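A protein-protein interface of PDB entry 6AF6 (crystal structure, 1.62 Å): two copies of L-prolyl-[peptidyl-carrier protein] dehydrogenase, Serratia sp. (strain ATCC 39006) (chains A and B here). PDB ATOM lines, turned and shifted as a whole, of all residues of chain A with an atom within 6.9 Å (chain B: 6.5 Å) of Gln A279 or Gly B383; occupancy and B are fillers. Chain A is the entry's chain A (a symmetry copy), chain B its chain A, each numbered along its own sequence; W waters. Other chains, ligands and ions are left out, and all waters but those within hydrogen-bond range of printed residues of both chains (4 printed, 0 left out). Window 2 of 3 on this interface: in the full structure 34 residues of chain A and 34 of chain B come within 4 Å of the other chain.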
ATOM      1  N   ALA A 267      -8.594 -10.119  21.179  1.00  0.00           N
ATOM      2  CA  ALA A 267      -9.213  -8.900  20.679  1.00  0.00           C
ATOM      3  C   ALA A 267      -8.455  -7.668  21.135  1.00  0.00           C
ATOM      4  O   ALA A 267      -8.537  -6.640  20.484  1.00  0.00           O
ATOM      5  CB  ALA A 267     -10.660  -8.798  21.131  1.00  0.00           C
ATOM      6  N   LYS A 275      -5.779  -0.206  14.956  1.00  0.00           N
ATOM      7  CA  LYS A 275      -6.195  -0.318  16.349  1.00  0.00           C
ATOM      8  C   LYS A 275      -6.516  -1.769  16.664  1.00  0.00           C
ATOM      9  O   LYS A 275      -6.655  -2.613  15.764  1.00  0.00           O
ATOM     10  CB  LYS A 275      -7.433   0.535  16.599  1.00  0.00           C
ATOM     11  CG  LYS A 275      -8.636   0.044  15.778  1.00  0.00           C
ATOM     12  CD  LYS A 275      -9.697   1.186  15.716  1.00  0.00           C
ATOM     13  CE  LYS A 275      -9.272   2.267  14.746  1.00  0.00           C
ATOM     14  NZ  LYS A 275     -10.056   3.531  14.933  1.00  0.00           N
ATOM     15  N   ALA A 276      -6.679  -2.046  17.936  1.00  0.00           N
ATOM     16  CA  ALA A 276      -7.104  -3.391  18.346  1.00  0.00           C
ATOM     17  C   ALA A 276      -8.501  -3.695  17.833  1.00  0.00           C
ATOM     18  O   ALA A 276      -9.366  -2.844  17.859  1.00  0.00           O
ATOM     19  CB  ALA A 276      -7.085  -3.534  19.867  1.00  0.00           C
ATOM     20  N   ILE A 277      -8.701  -4.934  17.355  1.00  0.00           N
ATOM     21  CA  ILE A 277     -10.015  -5.212  16.749  1.00  0.00           C
ATOM     22  C   ILE A 277     -11.121  -5.110  17.792  1.00  0.00           C
ATOM     23  O   ILE A 277     -12.267  -4.813  17.419  1.00  0.00           O
ATOM     24  CB  ILE A 277     -10.064  -6.612  16.086  1.00  0.00           C
ATOM     25  CG1 ILE A 277      -9.657  -7.682  17.083  1.00  0.00           C
ATOM     26  CG2 ILE A 277      -9.130  -6.629  14.841  1.00  0.00           C
ATOM     27  CD1 ILE A 277      -9.954  -9.163  16.518  1.00  0.00           C
ATOM     28  N   GLY A 278     -10.789  -5.259  19.069  1.00  0.00           N
ATOM     29  CA  GLY A 278     -11.826  -5.066  20.082  1.00  0.00           C
ATOM     30  C   GLY A 278     -12.362  -3.657  20.178  1.00  0.00           C
ATOM     31  O   GLY A 278     -13.445  -3.450  20.759  1.00  0.00           O
ATOM     32  N   GLN A 279     -11.706  -2.679  19.573  1.00  0.00           N
ATOM     33  CA  GLN A 279     -12.237  -1.316  19.552  1.00  0.00           C
ATOM     34  C   GLN A 279     -13.433  -1.119  18.637  1.00  0.00           C
ATOM     35  O   GLN A 279     -14.102  -0.094  18.776  1.00  0.00           O
ATOM     36  CB  GLN A 279     -11.131  -0.325  19.086  1.00  0.00           C
ATOM     37  CG  GLN A 279      -9.923  -0.353  20.047  1.00  0.00           C
ATOM     38  CD  GLN A 279      -9.912   0.715  21.061  1.00  0.00           C
ATOM     39  OE1 GLN A 279     -10.940   1.374  21.326  1.00  0.00           O
ATOM     40  NE2 GLN A 279      -8.757   0.907  21.669  1.00  0.00           N
ATOM     41  N   PHE A 280     -13.696  -2.034  17.667  1.00  0.00           N
ATOM     42  CA  PHE A 280     -14.856  -1.955  16.805  1.00  0.00           C
ATOM     43  C   PHE A 280     -16.039  -2.539  17.509  1.00  0.00           C
ATOM     44  O   PHE A 280     -15.936  -3.636  18.043  1.00  0.00           O
ATOM     45  CB  PHE A 280     -14.549  -2.772  15.552  1.00  0.00           C
ATOM     46  CG  PHE A 280     -13.430  -2.165  14.744  1.00  0.00           C
ATOM     47  CD1 PHE A 280     -13.672  -0.991  14.039  1.00  0.00           C
ATOM     48  CD2 PHE A 280     -12.228  -2.815  14.666  1.00  0.00           C
ATOM     49  CE1 PHE A 280     -12.660  -0.425  13.256  1.00  0.00           C
ATOM     50  CE2 PHE A 280     -11.172  -2.225  13.890  1.00  0.00           C
ATOM     51  CZ  PHE A 280     -11.422  -1.064  13.218  1.00  0.00           C
ATOM     52  N   GLN A 281     -17.152  -1.828  17.499  1.00  0.00           N
ATOM     53  CA  GLN A 281     -18.296  -2.337  18.275  1.00  0.00           C
ATOM     54  C   GLN A 281     -18.813  -3.662  17.727  1.00  0.00           C
ATOM     55  O   GLN A 281     -19.384  -4.451  18.495  1.00  0.00           O
ATOM     56  CB  GLN A 281     -19.424  -1.307  18.331  1.00  0.00           C
ATOM     57  CG  GLN A 281     -18.994  -0.117  19.240  1.00  0.00           C
ATOM     58  CD  GLN A 281     -19.931   1.060  19.141  1.00  0.00           C
ATOM     59  OE1 GLN A 281     -20.926   1.078  18.368  1.00  0.00           O
ATOM     60  NE2 GLN A 281     -19.626   2.118  19.918  1.00  0.00           N
ATOM     61  N   SER A 282     -18.675  -3.948  16.418  1.00  0.00           N
ATOM     62  CA  SER A 282     -19.125  -5.285  16.000  1.00  0.00           C
ATOM     63  C   SER A 282     -18.387  -6.381  16.761  1.00  0.00           C
ATOM     64  O   SER A 282     -18.965  -7.443  17.061  1.00  0.00           O
ATOM     65  CB  SER A 282     -18.867  -5.467  14.520  1.00  0.00           C
ATOM     66  OG  SER A 282     -19.802  -4.664  13.756  1.00  0.00           O
ATOM     67  N   VAL A 283     -17.102  -6.174  17.025  1.00  0.00           N
ATOM     68  CA  VAL A 283     -16.281  -7.165  17.719  1.00  0.00           C
ATOM     69  C   VAL A 283     -16.581  -7.161  19.205  1.00  0.00           C
ATOM     70  O   VAL A 283     -16.806  -8.219  19.795  1.00  0.00           O
ATOM     71  CB  VAL A 283     -14.803  -6.865  17.476  1.00  0.00           C
ATOM     72  CG1 VAL A 283     -13.898  -7.809  18.333  1.00  0.00           C
ATOM     73  CG2 VAL A 283     -14.549  -7.087  15.931  1.00  0.00           C
ATOM     74  N   SER A 284     -16.563  -5.981  19.796  1.00  0.00           N
ATOM     75  CA  SER A 284     -16.753  -5.933  21.247  1.00  0.00           C
ATOM     76  C   SER A 284     -18.168  -6.310  21.636  1.00  0.00           C
ATOM     77  O   SER A 284     -18.333  -6.992  22.653  1.00  0.00           O
ATOM     78  CB  SER A 284     -16.422  -4.548  21.841  1.00  0.00           C
ATOM     79  OG  SER A 284     -17.260  -3.526  21.290  1.00  0.00           O
ATOM     80  N   GLU B 373     -20.633   0.034  25.837  1.00  0.00           N
ATOM     81  CA  GLU B 373     -19.357   0.757  25.879  1.00  0.00           C
ATOM     82  C   GLU B 373     -18.751   0.704  27.258  1.00  0.00           C
ATOM     83  O   GLU B 373     -17.530   0.600  27.407  1.00  0.00           O
ATOM     84  CB  GLU B 373     -19.540   2.198  25.445  1.00  0.00           C
ATOM     85  CG  GLU B 373     -19.885   2.311  23.915  1.00  0.00           C
ATOM     86  CD  GLU B 373     -18.776   1.616  23.069  1.00  0.00           C
ATOM     87  OE1 GLU B 373     -17.663   2.130  23.018  1.00  0.00           O
ATOM     88  OE2 GLU B 373     -19.063   0.537  22.547  1.00  0.00           O
ATOM     89  N   ARG B 377     -15.175  -1.078  28.111  1.00  0.00           N
ATOM     90  CA  ARG B 377     -14.086  -0.384  28.819  1.00  0.00           C
ATOM     91  C   ARG B 377     -13.605  -1.218  30.015  1.00  0.00           C
ATOM     92  O   ARG B 377     -12.389  -1.374  30.224  1.00  0.00           O
ATOM     93  CB  ARG B 377     -14.546   0.989  29.248  1.00  0.00           C
ATOM     94  CG  ARG B 377     -13.414   1.723  30.029  1.00  0.00           C
ATOM     95  CD  ARG B 377     -13.728   3.207  30.173  1.00  0.00           C
ATOM     96  NE  ARG B 377     -15.113   3.419  30.652  1.00  0.00           N
ATOM     97  CZ  ARG B 377     -15.526   3.241  31.912  1.00  0.00           C
ATOM     98  NH1 ARG B 377     -14.664   2.836  32.846  1.00  0.00           N
ATOM     99  NH2 ARG B 377     -16.797   3.472  32.250  1.00  0.00           N
ATOM    100  N   GLY B 380     -11.360  -4.030  29.224  1.00  0.00           N
ATOM    101  CA  GLY B 380     -10.062  -3.697  28.611  1.00  0.00           C
ATOM    102  C   GLY B 380     -10.053  -3.553  27.118  1.00  0.00           C
ATOM    103  O   GLY B 380      -8.961  -3.550  26.511  1.00  0.00           O
ATOM    104  N   LEU B 381     -11.233  -3.431  26.477  1.00  0.00           N
ATOM    105  CA  LEU B 381     -11.337  -3.292  25.019  1.00  0.00           C
ATOM    106  C   LEU B 381     -11.350  -1.847  24.539  1.00  0.00           C
ATOM    107  O   LEU B 381     -11.602  -1.583  23.339  1.00  0.00           O
ATOM    108  CB  LEU B 381     -12.633  -3.995  24.516  1.00  0.00           C
ATOM    109  CG  LEU B 381     -12.629  -5.431  24.913  1.00  0.00           C
ATOM    110  CD1 LEU B 381     -14.009  -6.055  24.586  1.00  0.00           C
ATOM    111  CD2 LEU B 381     -11.523  -6.250  24.159  1.00  0.00           C
ATOM    112  N   ARG B 382     -11.080  -0.874  25.417  1.00  0.00           N
ATOM    113  CA  ARG B 382     -11.099   0.548  25.042  1.00  0.00           C
ATOM    114  C   ARG B 382      -9.767   1.187  25.461  1.00  0.00           C
ATOM    115  O   ARG B 382      -9.716   2.328  25.899  1.00  0.00           O
ATOM    116  CB  ARG B 382     -12.285   1.292  25.658  1.00  0.00           C
ATOM    117  CG  ARG B 382     -13.667   0.747  25.188  1.00  0.00           C
ATOM    118  CD  ARG B 382     -13.935   1.168  23.766  1.00  0.00           C
ATOM    119  NE  ARG B 382     -15.181   0.644  23.187  1.00  0.00           N
ATOM    120  CZ  ARG B 382     -15.286  -0.514  22.532  1.00  0.00           C
ATOM    121  NH1 ARG B 382     -16.449  -0.822  21.958  1.00  0.00           N
ATOM    122  NH2 ARG B 382     -14.245  -1.329  22.429  1.00  0.00           N
ATOM    123  N   GLY B 383      -8.689   0.426  25.321  1.00  0.00           N
ATOM    124  CA  GLY B 383      -7.383   0.783  25.900  1.00  0.00           C
ATOM    125  C   GLY B 383      -6.561   1.744  25.054  1.00  0.00           C
ATOM    126  O   GLY B 383      -7.125   2.503  24.260  1.00  0.00           O
HETATM  127  O   HOH W   1     -13.377   1.886  20.677  1.00  0.00           O
HETATM  128  O   HOH W   2     -16.625   3.235  20.675  1.00  0.00           O
HETATM  129  O   HOH W   3     -19.350  -2.738  22.496  1.00  0.00           O
HETATM  130  O   HOH W   4      -9.708  -3.667  22.164  1.00  0.00           O
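The side-chain amide nitrogen of Gln A281 lies within hydrogen-bond range of the side-chain carboxylate of Glu B373 (3.1 Å).
The backbone carbonyl oxygen (O) of Gly B383 is in hydrogen-bond range of the side-chain amide nitrogen (NE2) of Gln A279, 3.5 Å away.
NH1 of Arg B382 lies within hydrogen-bond range of OG of Ser A284, 2.9 Å away.
The guanidinium group (NH2) of Arg B382 is in hydrogen-bond range of the backbone carbonyl oxygen (O) of Gly A278 (2.8 Å).
N of Gly A278 is in hydrogen-bond range of O of Ala A267 (3.0 Å).
OE1 of Glu B373 is in salt-bridge range of NE of Arg B382 (2.9 Å).
Gly A278 touches Leu B381 (O to O, 3.7 Å).
OE1 of Gln A279 touches O of Leu B381, at 3.6 Å.
NH2 of Arg B382 touches CA of Gln A279 (3.5 Å).
Gln A281 touches Arg B382.
Ser A284 touches Leu B381.
Gln A279 touches three residues of chain B.
Of the printed residues of chain B, Ser A284 touches Leu B381 (3.95 Å) and Arg B382 (2.9 Å).
Of the printed residues of chain A, Glu B373 touches Gln A281.
Arg B377 touches none of the printed residues of chain A.
Of the printed residues of chain A, Gly B383 touches Gln A279.
The nearest printed residue of chain A that does not touch Gly B383 is Ala A276 (6.9 Å).
The nearest printed residue of chain A that does not touch Arg B382 is Phe A280 (4.8 Å).
Of the 11 printed residues of chain A, 4 touch a printed residue of chain B.
Hydrophobic or aromatic side chains of chain B that line the printed part of chain A: Leu B381.
Among the printed residues, 9 pairs touch across the chains.
No position is printed for both chains.
Of the 9 pairs that touch across the chains among the printed residues, none has its exchanged pair printed and touching as well.
Water W3 bridges OG of Ser A284 (2.5 Å) and OE2 of Glu B373 (3.3 Å).
Water W1 bridges OE1 of Gln A279 (2.6 Å) and NE of Arg B382 (3.3 Å).
Water W2 bridges OE1 of Glu B373 and NE2 of Gln A281.
Water W4 bridges the backbone carbonyl oxygen (O) of Leu B381 (3.1 Å) and the backbone NH (N) of Gln A279 (3.4 Å).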
